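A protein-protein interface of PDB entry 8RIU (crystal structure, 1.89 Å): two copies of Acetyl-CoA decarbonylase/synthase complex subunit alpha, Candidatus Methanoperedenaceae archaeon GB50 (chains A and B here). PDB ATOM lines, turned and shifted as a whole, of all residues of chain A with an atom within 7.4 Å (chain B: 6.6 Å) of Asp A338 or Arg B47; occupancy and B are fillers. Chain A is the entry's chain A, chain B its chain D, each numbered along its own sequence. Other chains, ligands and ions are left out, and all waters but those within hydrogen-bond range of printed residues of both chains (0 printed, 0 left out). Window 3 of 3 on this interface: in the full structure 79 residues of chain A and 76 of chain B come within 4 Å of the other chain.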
ATOM      1  N   ALA A 327      20.713 -27.754  -0.950  1.00  0.00           N
ATOM      2  CA  ALA A 327      21.985 -27.099  -1.225  1.00  0.00           C
ATOM      3  C   ALA A 327      21.861 -25.613  -0.909  1.00  0.00           C
ATOM      4  O   ALA A 327      20.935 -24.947  -1.385  1.00  0.00           O
ATOM      5  CB  ALA A 327      22.396 -27.307  -2.682  1.00  0.00           C
ATOM      6  N   ALA A 332      28.202 -25.094  -5.040  1.00  0.00           N
ATOM      7  CA  ALA A 332      27.766 -26.472  -5.248  1.00  0.00           C
ATOM      8  C   ALA A 332      26.248 -26.468  -5.417  1.00  0.00           C
ATOM      9  O   ALA A 332      25.507 -26.473  -4.424  1.00  0.00           O
ATOM     10  CB  ALA A 332      28.193 -27.351  -4.080  1.00  0.00           C
ATOM     11  N   LEU A 333      25.786 -26.498  -6.673  1.00  0.00           N
ATOM     12  CA  LEU A 333      24.325 -26.443  -6.966  1.00  0.00           C
ATOM     13  C   LEU A 333      23.830 -27.799  -7.480  1.00  0.00           C
ATOM     14  O   LEU A 333      22.634 -28.079  -7.297  1.00  0.00           O
ATOM     15  CB  LEU A 333      24.084 -25.333  -7.990  1.00  0.00           C
ATOM     16  CG  LEU A 333      24.576 -23.950  -7.568  1.00  0.00           C
ATOM     17  CD1 LEU A 333      24.665 -23.017  -8.764  1.00  0.00           C
ATOM     18  CD2 LEU A 333      23.677 -23.360  -6.490  1.00  0.00           C
ATOM     19  N   TYR A 334      24.691 -28.586  -8.132  1.00  0.00           N
ATOM     20  CA  TYR A 334      24.322 -29.944  -8.531  1.00  0.00           C
ATOM     21  C   TYR A 334      23.182 -29.973  -9.545  1.00  0.00           C
ATOM     22  O   TYR A 334      22.434 -30.950  -9.612  1.00  0.00           O
ATOM     23  CB  TYR A 334      23.938 -30.790  -7.314  1.00  0.00           C
ATOM     24  CG  TYR A 334      24.900 -30.714  -6.148  1.00  0.00           C
ATOM     25  CD1 TYR A 334      26.095 -31.426  -6.153  1.00  0.00           C
ATOM     26  CD2 TYR A 334      24.601 -29.955  -5.028  1.00  0.00           C
ATOM     27  CE1 TYR A 334      26.967 -31.366  -5.074  1.00  0.00           C
ATOM     28  CE2 TYR A 334      25.464 -29.892  -3.953  1.00  0.00           C
ATOM     29  CZ  TYR A 334      26.641 -30.601  -3.979  1.00  0.00           C
ATOM     30  OH  TYR A 334      27.493 -30.528  -2.896  1.00  0.00           O
ATOM     31  N   GLY A 335      23.035 -28.920 -10.347  1.00  0.00           N
ATOM     32  CA  GLY A 335      21.974 -28.886 -11.337  1.00  0.00           C
ATOM     33  C   GLY A 335      20.590 -28.646 -10.778  1.00  0.00           C
ATOM     34  O   GLY A 335      19.605 -28.726 -11.520  1.00  0.00           O
ATOM     35  N   LEU A 336      20.485 -28.337  -9.496  1.00  0.00           N
ATOM     36  CA  LEU A 336      19.188 -28.174  -8.867  1.00  0.00           C
ATOM     37  C   LEU A 336      18.608 -26.800  -9.178  1.00  0.00           C
ATOM     38  O   LEU A 336      19.322 -25.862  -9.541  1.00  0.00           O
ATOM     39  CB  LEU A 336      19.324 -28.373  -7.360  1.00  0.00           C
ATOM     40  CG  LEU A 336      19.718 -29.796  -6.980  1.00  0.00           C
ATOM     41  CD1 LEU A 336      19.945 -29.892  -5.474  1.00  0.00           C
ATOM     42  CD2 LEU A 336      18.644 -30.782  -7.434  1.00  0.00           C
ATOM     43  N   VAL A 337      17.293 -26.688  -9.035  1.00  0.00           N
ATOM     44  CA  VAL A 337      16.613 -25.424  -9.286  1.00  0.00           C
ATOM     45  C   VAL A 337      16.870 -24.487  -8.114  1.00  0.00           C
ATOM     46  O   VAL A 337      16.770 -24.887  -6.947  1.00  0.00           O
ATOM     47  CB  VAL A 337      15.108 -25.641  -9.503  1.00  0.00           C
ATOM     48  CG1 VAL A 337      14.441 -24.322  -9.905  1.00  0.00           C
ATOM     49  CG2 VAL A 337      14.864 -26.708 -10.561  1.00  0.00           C
ATOM     50  N   ASP A 338      17.209 -23.238  -8.425  1.00  0.00           N
ATOM     51  CA  ASP A 338      17.385 -22.200  -7.412  1.00  0.00           C
ATOM     52  C   ASP A 338      16.009 -21.711  -6.979  1.00  0.00           C
ATOM     53  O   ASP A 338      15.355 -20.944  -7.688  1.00  0.00           O
ATOM     54  CB  ASP A 338      18.223 -21.052  -7.960  1.00  0.00           C
ATOM     55  CG  ASP A 338      18.385 -19.920  -6.965  1.00  0.00           C
ATOM     56  OD1 ASP A 338      17.899 -20.049  -5.820  1.00  0.00           O
ATOM     57  OD2 ASP A 338      18.992 -18.892  -7.334  1.00  0.00           O
ATOM     58  N   ARG A 339      15.578 -22.137  -5.795  1.00  0.00           N
ATOM     59  CA  ARG A 339      14.278 -21.766  -5.248  1.00  0.00           C
ATOM     60  C   ARG A 339      14.420 -20.813  -4.065  1.00  0.00           C
ATOM     61  O   ARG A 339      13.592 -20.809  -3.149  1.00  0.00           O
ATOM     62  CB  ARG A 339      13.506 -23.024  -4.852  1.00  0.00           C
ATOM     63  CG  ARG A 339      13.234 -23.952  -6.032  1.00  0.00           C
ATOM     64  CD  ARG A 339      12.025 -24.843  -5.803  1.00  0.00           C
ATOM     65  NE  ARG A 339      11.672 -25.569  -7.019  1.00  0.00           N
ATOM     66  CZ  ARG A 339      10.976 -25.055  -8.024  1.00  0.00           C
ATOM     67  NH1 ARG A 339      10.516 -23.815  -7.985  1.00  0.00           N
ATOM     68  NH2 ARG A 339      10.737 -25.801  -9.097  1.00  0.00           N
ATOM     69  N   THR A 340      15.467 -19.989  -4.088  1.00  0.00           N
ATOM     70  CA  THR A 340      15.694 -19.028  -3.015  1.00  0.00           C
ATOM     71  C   THR A 340      14.484 -18.123  -2.806  1.00  0.00           C
ATOM     72  O   THR A 340      14.169 -17.757  -1.667  1.00  0.00           O
ATOM     73  CB  THR A 340      16.944 -18.199  -3.331  1.00  0.00           C
ATOM     74  OG1 THR A 340      18.075 -19.072  -3.452  1.00  0.00           O
ATOM     75  CG2 THR A 340      17.218 -17.166  -2.248  1.00  0.00           C
ATOM     76  N   ASP A 341      13.792 -17.755  -3.887  1.00  0.00           N
ATOM     77  CA  ASP A 341      12.683 -16.811  -3.820  1.00  0.00           C
ATOM     78  C   ASP A 341      11.332 -17.474  -3.599  1.00  0.00           C
ATOM     79  O   ASP A 341      10.331 -16.766  -3.444  1.00  0.00           O
ATOM     80  CB  ASP A 341      12.612 -15.983  -5.106  1.00  0.00           C
ATOM     81  CG  ASP A 341      13.831 -15.105  -5.301  1.00  0.00           C
ATOM     82  OD1 ASP A 341      14.385 -14.618  -4.287  1.00  0.00           O
ATOM     83  OD2 ASP A 341      14.241 -14.913  -6.468  1.00  0.00           O
ATOM     84  N   ASP A 342      11.268 -18.800  -3.593  1.00  0.00           N
ATOM     85  CA  ASP A 342       9.996 -19.476  -3.401  1.00  0.00           C
ATOM     86  C   ASP A 342       9.650 -19.551  -1.916  1.00  0.00           C
ATOM     87  O   ASP A 342      10.518 -19.499  -1.041  1.00  0.00           O
ATOM     88  CB  ASP A 342      10.036 -20.881  -4.001  1.00  0.00           C
ATOM     89  CG  ASP A 342       9.953 -20.872  -5.514  1.00  0.00           C
ATOM     90  OD1 ASP A 342       9.130 -20.111  -6.065  1.00  0.00           O
ATOM     91  OD2 ASP A 342      10.714 -21.627  -6.153  1.00  0.00           O
ATOM     92  N   ILE A 347       8.357 -24.972  -1.340  1.00  0.00           N
ATOM     93  CA  ILE A 347       9.541 -25.819  -1.428  1.00  0.00           C
ATOM     94  C   ILE A 347       9.272 -27.168  -0.772  1.00  0.00           C
ATOM     95  O   ILE A 347       9.610 -28.222  -1.321  1.00  0.00           O
ATOM     96  CB  ILE A 347      10.752 -25.112  -0.795  1.00  0.00           C
ATOM     97  CG1 ILE A 347      11.235 -23.977  -1.705  1.00  0.00           C
ATOM     98  CG2 ILE A 347      11.884 -26.108  -0.540  1.00  0.00           C
ATOM     99  CD1 ILE A 347      11.916 -22.859  -0.969  1.00  0.00           C
ATOM    100  N   GLU A 356      11.050 -33.172  -7.348  1.00  0.00           N
ATOM    101  CA  GLU A 356      12.442 -32.747  -7.446  1.00  0.00           C
ATOM    102  C   GLU A 356      13.200 -33.423  -6.310  1.00  0.00           C
ATOM    103  O   GLU A 356      12.704 -33.455  -5.172  1.00  0.00           O
ATOM    104  CB  GLU A 356      12.574 -31.221  -7.358  1.00  0.00           C
ATOM    105  CG  GLU A 356      12.116 -30.506  -8.618  1.00  0.00           C
ATOM    106  CD  GLU A 356      12.001 -29.000  -8.445  1.00  0.00           C
ATOM    107  OE1 GLU A 356      12.661 -28.440  -7.538  1.00  0.00           O
ATOM    108  OE2 GLU A 356      11.243 -28.376  -9.221  1.00  0.00           O
ATOM    109  N   VAL A 359      16.772 -29.083  -3.827  1.00  0.00           N
ATOM    110  CA  VAL A 359      16.614 -27.687  -4.218  1.00  0.00           C
ATOM    111  C   VAL A 359      17.830 -26.897  -3.759  1.00  0.00           C
ATOM    112  O   VAL A 359      18.555 -27.298  -2.847  1.00  0.00           O
ATOM    113  CB  VAL A 359      15.337 -27.047  -3.623  1.00  0.00           C
ATOM    114  CG1 VAL A 359      14.091 -27.683  -4.204  1.00  0.00           C
ATOM    115  CG2 VAL A 359      15.352 -27.184  -2.123  1.00  0.00           C
ATOM    116  N   VAL A 360      18.041 -25.752  -4.398  1.00  0.00           N
ATOM    117  CA  VAL A 360      19.015 -24.767  -3.951  1.00  0.00           C
ATOM    118  C   VAL A 360      18.261 -23.670  -3.211  1.00  0.00           C
ATOM    119  O   VAL A 360      17.255 -23.147  -3.711  1.00  0.00           O
ATOM    120  CB  VAL A 360      19.814 -24.195  -5.133  1.00  0.00           C
ATOM    121  CG1 VAL A 360      20.479 -22.860  -4.754  1.00  0.00           C
ATOM    122  CG2 VAL A 360      20.845 -25.196  -5.595  1.00  0.00           C
ATOM    123  N   ILE A 361      18.731 -23.331  -2.015  1.00  0.00           N
ATOM    124  CA  ILE A 361      18.174 -22.243  -1.222  1.00  0.00           C
ATOM    125  C   ILE A 361      19.358 -21.448  -0.695  1.00  0.00           C
ATOM    126  O   ILE A 361      20.006 -21.859   0.274  1.00  0.00           O
ATOM    127  CB  ILE A 361      17.293 -22.737  -0.073  1.00  0.00           C
ATOM    128  CG1 ILE A 361      16.141 -23.585  -0.614  1.00  0.00           C
ATOM    129  CG2 ILE A 361      16.759 -21.539   0.716  1.00  0.00           C
ATOM    130  CD1 ILE A 361      15.489 -24.474   0.436  1.00  0.00           C
ATOM    131  N   LEU A 362      19.636 -20.309  -1.318  1.00  0.00           N
ATOM    132  CA  LEU A 362      20.767 -19.467  -0.960  1.00  0.00           C
ATOM    133  C   LEU A 362      20.440 -18.496   0.169  1.00  0.00           C
ATOM    134  O   LEU A 362      21.326 -17.764   0.624  1.00  0.00           O
ATOM    135  CB  LEU A 362      21.236 -18.706  -2.202  1.00  0.00           C
ATOM    136  CG  LEU A 362      21.632 -19.601  -3.383  1.00  0.00           C
ATOM    137  CD1 LEU A 362      22.282 -18.786  -4.483  1.00  0.00           C
ATOM    138  CD2 LEU A 362      22.563 -20.735  -2.957  1.00  0.00           C
ATOM    139  N   ASP A 363      19.189 -18.483   0.625  1.00  0.00           N
ATOM    140  CA  ASP A 363      18.777 -17.722   1.796  1.00  0.00           C
ATOM    141  C   ASP A 363      18.884 -18.651   3.001  1.00  0.00           C
ATOM    142  O   ASP A 363      18.105 -19.610   3.096  1.00  0.00           O
ATOM    143  CB  ASP A 363      17.346 -17.223   1.609  1.00  0.00           C
ATOM    144  CG  ASP A 363      16.756 -16.586   2.858  1.00  0.00           C
ATOM    145  OD1 ASP A 363      17.385 -16.624   3.936  1.00  0.00           O
ATOM    146  OD2 ASP A 363      15.629 -16.056   2.756  1.00  0.00           O
ATOM    147  N   GLY B  42      26.551 -12.622  -9.156  1.00  0.00           N
ATOM    148  CA  GLY B  42      27.348 -13.709  -8.576  1.00  0.00           C
ATOM    149  C   GLY B  42      27.168 -14.946  -9.440  1.00  0.00           C
ATOM    150  O   GLY B  42      26.552 -14.825 -10.501  1.00  0.00           O
ATOM    151  N   ILE B  43      27.652 -16.102  -9.001  1.00  0.00           N
ATOM    152  CA  ILE B  43      27.618 -17.346  -9.831  1.00  0.00           C
ATOM    153  C   ILE B  43      26.207 -17.687 -10.334  1.00  0.00           C
ATOM    154  O   ILE B  43      26.094 -18.056 -11.496  1.00  0.00           O
ATOM    155  CB  ILE B  43      28.225 -18.513  -9.026  1.00  0.00           C
ATOM    156  CG1 ILE B  43      29.721 -18.307  -8.776  1.00  0.00           C
ATOM    157  CG2 ILE B  43      27.943 -19.848  -9.695  1.00  0.00           C
ATOM    158  CD1 ILE B  43      30.211 -18.900  -7.478  1.00  0.00           C
ATOM    159  N   VAL B  44      25.180 -17.576  -9.492  1.00  0.00           N
ATOM    160  CA  VAL B  44      23.805 -18.030  -9.870  1.00  0.00           C
ATOM    161  C   VAL B  44      23.006 -16.940 -10.590  1.00  0.00           C
ATOM    162  O   VAL B  44      22.009 -17.283 -11.215  1.00  0.00           O
ATOM    163  CB  VAL B  44      23.052 -18.496  -8.612  1.00  0.00           C
ATOM    164  CG1 VAL B  44      23.706 -19.711  -7.978  1.00  0.00           C
ATOM    165  CG2 VAL B  44      22.885 -17.378  -7.597  1.00  0.00           C
ATOM    166  N   ASP B  45      23.447 -15.690 -10.537  1.00  0.00           N
ATOM    167  CA  ASP B  45      22.643 -14.558 -11.068  1.00  0.00           C
ATOM    168  C   ASP B  45      22.431 -14.648 -12.587  1.00  0.00           C
ATOM    169  O   ASP B  45      21.404 -14.158 -13.056  1.00  0.00           O
ATOM    170  CB  ASP B  45      23.254 -13.248 -10.570  1.00  0.00           C
ATOM    171  CG  ASP B  45      23.113 -13.085  -9.069  1.00  0.00           C
ATOM    172  OD1 ASP B  45      22.068 -13.489  -8.540  1.00  0.00           O
ATOM    173  OD2 ASP B  45      24.047 -12.566  -8.446  1.00  0.00           O
ATOM    174  N   LEU B  46      23.368 -15.244 -13.322  1.00  0.00           N
ATOM    175  CA  LEU B  46      23.216 -15.394 -14.768  1.00  0.00           C
ATOM    176  C   LEU B  46      23.225 -16.866 -15.180  1.00  0.00           C
ATOM    177  O   LEU B  46      23.415 -17.183 -16.358  1.00  0.00           O
ATOM    178  CB  LEU B  46      24.313 -14.617 -15.498  1.00  0.00           C
ATOM    179  CG  LEU B  46      24.119 -13.096 -15.497  1.00  0.00           C
ATOM    180  CD1 LEU B  46      25.334 -12.375 -16.082  1.00  0.00           C
ATOM    181  CD2 LEU B  46      22.863 -12.698 -16.259  1.00  0.00           C
ATOM    182  N   ARG B  47      23.012 -17.767 -14.220  1.00  0.00           N
ATOM    183  CA  ARG B  47      23.020 -19.201 -14.498  1.00  0.00           C
ATOM    184  C   ARG B  47      21.926 -19.590 -15.487  1.00  0.00           C
ATOM    185  O   ARG B  47      22.124 -20.476 -16.327  1.00  0.00           O
ATOM    186  CB  ARG B  47      22.854 -19.949 -13.174  1.00  0.00           C
ATOM    187  CG  ARG B  47      22.737 -21.464 -13.237  1.00  0.00           C
ATOM    188  CD  ARG B  47      22.649 -21.977 -11.813  1.00  0.00           C
ATOM    189  NE  ARG B  47      22.525 -23.422 -11.697  1.00  0.00           N
ATOM    190  CZ  ARG B  47      21.579 -24.045 -11.006  1.00  0.00           C
ATOM    191  NH1 ARG B  47      20.554 -23.394 -10.488  1.00  0.00           N
ATOM    192  NH2 ARG B  47      21.665 -25.360 -10.831  1.00  0.00           N
ATOM    193  N   ASP B  48      20.760 -18.949 -15.400  1.00  0.00           N
ATOM    194  CA  ASP B  48      19.668 -19.312 -16.297  1.00  0.00           C
ATOM    195  C   ASP B  48      19.978 -18.929 -17.740  1.00  0.00           C
ATOM    196  O   ASP B  48      19.583 -19.646 -18.665  1.00  0.00           O
ATOM    197  CB  ASP B  48      18.370 -18.662 -15.823  1.00  0.00           C
ATOM    198  CG  ASP B  48      17.938 -19.160 -14.456  1.00  0.00           C
ATOM    199  OD1 ASP B  48      18.355 -20.281 -14.074  1.00  0.00           O
ATOM    200  OD2 ASP B  48      17.188 -18.434 -13.762  1.00  0.00           O
ATOM    201  N   TRP B  49      20.690 -17.820 -17.959  1.00  0.00           N
ATOM    202  CA  TRP B  49      21.131 -17.500 -19.314  1.00  0.00           C
ATOM    203  C   TRP B  49      22.139 -18.526 -19.816  1.00  0.00           C
ATOM    204  O   TRP B  49      22.053 -18.976 -20.963  1.00  0.00           O
ATOM    205  CB  TRP B  49      21.730 -16.093 -19.369  1.00  0.00           C
ATOM    206  CG  TRP B  49      22.465 -15.833 -20.653  1.00  0.00           C
ATOM    207  CD1 TRP B  49      23.810 -15.630 -20.809  1.00  0.00           C
ATOM    208  CD2 TRP B  49      21.896 -15.770 -21.963  1.00  0.00           C
ATOM    209  NE1 TRP B  49      24.108 -15.437 -22.137  1.00  0.00           N
ATOM    210  CE2 TRP B  49      22.951 -15.522 -22.866  1.00  0.00           C
ATOM    211  CE3 TRP B  49      20.598 -15.898 -22.461  1.00  0.00           C
ATOM    212  CZ2 TRP B  49      22.744 -15.399 -24.236  1.00  0.00           C
ATOM    213  CZ3 TRP B  49      20.396 -15.776 -23.820  1.00  0.00           C
ATOM    214  CH2 TRP B  49      21.465 -15.528 -24.693  1.00  0.00           C
ATOM    215  N   ASP B  50      23.079 -18.939 -18.971  1.00  0.00           N
ATOM    216  CA  ASP B  50      24.073 -19.974 -19.375  1.00  0.00           C
ATOM    217  C   ASP B  50      23.361 -21.256 -19.846  1.00  0.00           C
ATOM    218  O   ASP B  50      23.791 -21.853 -20.848  1.00  0.00           O
ATOM    219  CB  ASP B  50      25.085 -20.221 -18.253  1.00  0.00           C
ATOM    220  CG  ASP B  50      25.978 -19.033 -17.949  1.00  0.00           C
ATOM    221  OD1 ASP B  50      26.068 -18.138 -18.800  1.00  0.00           O
ATOM    222  OD2 ASP B  50      26.577 -19.021 -16.865  1.00  0.00           O
ATOM    223  N   TYR B  51      22.293 -21.643 -19.158  1.00  0.00           N
ATOM    224  CA  TYR B  51      21.563 -22.885 -19.526  1.00  0.00           C
ATOM    225  C   TYR B  51      20.862 -22.693 -20.871  1.00  0.00           C
ATOM    226  O   TYR B  51      20.700 -23.661 -21.610  1.00  0.00           O
ATOM    227  CB  TYR B  51      20.580 -23.280 -18.430  1.00  0.00           C
ATOM    228  CG  TYR B  51      21.091 -24.147 -17.310  1.00  0.00           C
ATOM    229  CD1 TYR B  51      22.065 -23.701 -16.434  1.00  0.00           C
ATOM    230  CD2 TYR B  51      20.560 -25.406 -17.096  1.00  0.00           C
ATOM    231  CE1 TYR B  51      22.516 -24.494 -15.392  1.00  0.00           C
ATOM    232  CE2 TYR B  51      20.999 -26.213 -16.063  1.00  0.00           C
ATOM    233  CZ  TYR B  51      21.982 -25.756 -15.207  1.00  0.00           C
ATOM    234  OH  TYR B  51      22.411 -26.563 -14.187  1.00  0.00           O
ATOM    235  N   LYS B  52      20.470 -21.462 -21.175  1.00  0.00           N
ATOM    236  CA  LYS B  52      19.894 -21.182 -22.510  1.00  0.00           C
ATOM    237  C   LYS B  52      20.990 -21.453 -23.542  1.00  0.00           C
ATOM    238  O   LYS B  52      20.715 -22.106 -24.543  1.00  0.00           O
ATOM    239  CB  LYS B  52      19.385 -19.740 -22.562  1.00  0.00           C
ATOM    240  CG  LYS B  52      18.196 -19.434 -21.667  1.00  0.00           C
ATOM    241  CD  LYS B  52      16.874 -19.610 -22.368  1.00  0.00           C
ATOM    242  CE  LYS B  52      15.689 -19.332 -21.470  1.00  0.00           C
ATOM    243  NZ  LYS B  52      14.446 -19.912 -22.027  1.00  0.00           N
ATOM    244  N   MET B  54      23.637 -23.437 -23.096  1.00  0.00           N
ATOM    245  CA  MET B  54      24.104 -24.820 -23.056  1.00  0.00           C
ATOM    246  C   MET B  54      23.018 -25.813 -23.452  1.00  0.00           C
ATOM    247  O   MET B  54      23.338 -26.918 -23.908  1.00  0.00           O
ATOM    248  CB  MET B  54      24.641 -25.149 -21.659  1.00  0.00           C
ATOM    249  CG  MET B  54      26.115 -24.788 -21.498  1.00  0.00           C
ATOM    250  SD  MET B  54      26.823 -25.076 -19.862  1.00  0.00           S
ATOM    251  CE  MET B  54      25.624 -24.273 -18.784  1.00  0.00           C
ATOM    252  N   GLU B 179      31.158 -28.262  -6.480  1.00  0.00           N
ATOM    253  CA  GLU B 179      30.222 -28.532  -7.568  1.00  0.00           C
ATOM    254  C   GLU B 179      30.320 -29.960  -8.089  1.00  0.00           C
ATOM    255  O   GLU B 179      31.416 -30.471  -8.351  1.00  0.00           O
ATOM    256  CB  GLU B 179      30.440 -27.536  -8.713  1.00  0.00           C
ATOM    257  CG  GLU B 179      29.336 -27.500  -9.756  1.00  0.00           C
ATOM    258  CD  GLU B 179      27.958 -27.375  -9.160  1.00  0.00           C
ATOM    259  OE1 GLU B 179      27.593 -26.253  -8.731  1.00  0.00           O
ATOM    260  OE2 GLU B 179      27.237 -28.399  -9.117  1.00  0.00           O
ATOM    261  N   SER B 181      27.817 -30.925 -10.598  1.00  0.00           N
ATOM    262  CA  SER B 181      27.219 -30.855 -11.954  1.00  0.00           C
ATOM    263  C   SER B 181      28.211 -30.237 -12.935  1.00  0.00           C
ATOM    264  O   SER B 181      28.652 -29.122 -12.682  1.00  0.00           O
ATOM    265  CB  SER B 181      25.922 -30.082 -11.983  1.00  0.00           C
ATOM    266  OG  SER B 181      25.583 -29.732 -13.312  1.00  0.00           O
ATOM    267  N   ASP B 184      26.844 -26.874 -14.201  1.00  0.00           N
ATOM    268  CA  ASP B 184      27.019 -25.740 -13.260  1.00  0.00           C
ATOM    269  C   ASP B 184      28.487 -25.288 -13.281  1.00  0.00           C
ATOM    270  O   ASP B 184      28.740 -24.106 -13.083  1.00  0.00           O
ATOM    271  CB  ASP B 184      26.421 -26.094 -11.895  1.00  0.00           C
ATOM    272  CG  ASP B 184      24.902 -26.109 -11.914  1.00  0.00           C
ATOM    273  OD1 ASP B 184      24.330 -25.582 -12.877  1.00  0.00           O
ATOM    274  OD2 ASP B 184      24.310 -26.647 -10.970  1.00  0.00           O
ATOM    275  N   SER B 187      28.806 -23.184 -16.277  1.00  0.00           N
ATOM    276  CA  SER B 187      28.209 -21.874 -15.920  1.00  0.00           C
ATOM    277  C   SER B 187      29.236 -21.060 -15.139  1.00  0.00           C
ATOM    278  O   SER B 187      29.395 -19.877 -15.421  1.00  0.00           O
ATOM    279  CB  SER B 187      26.926 -22.023 -15.151  1.00  0.00           C
ATOM    280  OG  SER B 187      26.287 -20.772 -14.978  1.00  0.00           O
ATOM    281  N   ARG B 632      29.671 -16.052 -23.736  1.00  0.00           N
ATOM    282  CA  ARG B 632      28.550 -15.728 -22.858  1.00  0.00           C
ATOM    283  C   ARG B 632      27.761 -14.534 -23.367  1.00  0.00           C
ATOM    284  O   ARG B 632      26.538 -14.482 -23.189  1.00  0.00           O
ATOM    285  CB  ARG B 632      29.029 -15.456 -21.434  1.00  0.00           C
ATOM    286  CG  ARG B 632      27.933 -15.671 -20.396  1.00  0.00           C
ATOM    287  CD  ARG B 632      28.330 -15.183 -18.994  1.00  0.00           C
ATOM    288  NE  ARG B 632      27.733 -16.016 -17.954  1.00  0.00           N
ATOM    289  CZ  ARG B 632      27.656 -15.693 -16.670  1.00  0.00           C
ATOM    290  NH1 ARG B 632      28.060 -14.515 -16.225  1.00  0.00           N
ATOM    291  NH2 ARG B 632      27.178 -16.582 -15.805  1.00  0.00           N
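No position is printed for both chains.
Of the 15 pairs that touch across the chains among the printed residues, none has its exchanged pair printed and touching as well.
Of the 19 printed residues of chain A, 7 touch a printed residue of chain B.
Printed residues of chain A that touch a printed residue of chain B: Ala A332, Leu A333, Tyr A334, Gly A335, Leu A336, Asp A338 and Leu A362.
Of the 17 printed residues of chain B, 6 touch a printed residue of chain A.
Hydrophobic or aromatic side chains of chain B that line the printed part of chain A: Val B44 and Tyr B51.
Among the printed residues, no Asp or Glu carboxylate lies within 4 Å of a Lys or Arg side-chain nitrogen of the other chain.
Asp A338 touches just one residue of chain B: Arg B47.
Arg B47 touches just these residues of chain A: Leu A333, Gly A335, Leu A336 and Asp A338.
Of the printed residues of chain B, Ala A332 touches Glu B179.
Of the printed residues of chain B, Leu A362 touches Val B44.
Printed residues of chain B within 4 Å of Leu A333: Val B44 (3.5 Å), Arg B47 (3.7 Å), Glu B179 (2.7 Å) and Asp B184 (3.3 Å).
Printed residues of chain A within 4 Å of Ser B181: Tyr A334 and Gly A335.
Of the printed residues of chain A, Glu B179 touches Ala A332, Leu A333 and Tyr A334.
Ile B43 touches none of the printed residues of chain A.
Ser B187 touches none of the printed residues of chain A.
The nearest residue of chain A that does not touch Arg B47 is Val A337 (4.5 Å).
OE1 of Glu B179 touches CA of Ala A332, at 3.5 Å.
Val B44 touches Leu A333.
Leu A333 touches Arg B47 (CD1 to NE, 3.7 Å).
OD2 of Asp B184 touches CB of Leu A333, 3.3 Å away.
Tyr A334 touches Ser B181.
Gly A335 touches Arg B47 (C to NH2, 3.5 Å).
Gly A335 touches Tyr B51 (CA to OH, 3.7 Å).
CB of Ser B181 touches N of Gly A335, at 3.5 Å.
NH1 of Arg B47 touches N of Asp A338, at 3.9 Å.
CG2 of Val B44 touches CD1 of Leu A362 (3.5 Å).
OD1 of Asp A338 lies within hydrogen-bond range of OG1 of Thr A340, at 2.6 Å.
The backbone NH (N) of Leu A362 sits at hydrogen-bond distance from the side-chain hydroxyl (OG1) of Thr A340 (2.9 Å).
NH2 of Arg B47 lies within salt-bridge range of OD2 of Asp B184 (2.9 Å).
The side-chain hydroxyl of Tyr B51 is in hydrogen-bond range of the side-chain carboxylate of Asp B184, 2.5 Å away.
OE2 of Glu B179 is in hydrogen-bond range of N of Ser B181 (3.0 Å).
The side-chain hydroxyl of Ser B181 is in hydrogen-bond range of the backbone NH of Asp B184 (3.2 Å).
N of Leu A333 lies within hydrogen-bond range of OE1 of Glu B179 (2.7 Å).
The backbone NH (N) of Tyr A334 is in hydrogen-bond range of the side-chain carboxylate (OE2) of Glu B179, at 2.7 Å.
The backbone NH of Tyr A334 lies within hydrogen-bond range of the side-chain carboxylate of Asp B184.
The side-chain carboxylate of Asp B184 is in hydrogen-bond range of the backbone NH of Gly A335 (2.7 Å).
O of Leu A336 is in hydrogen-bond range of NH2 of Arg B47, at 2.7 Å.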
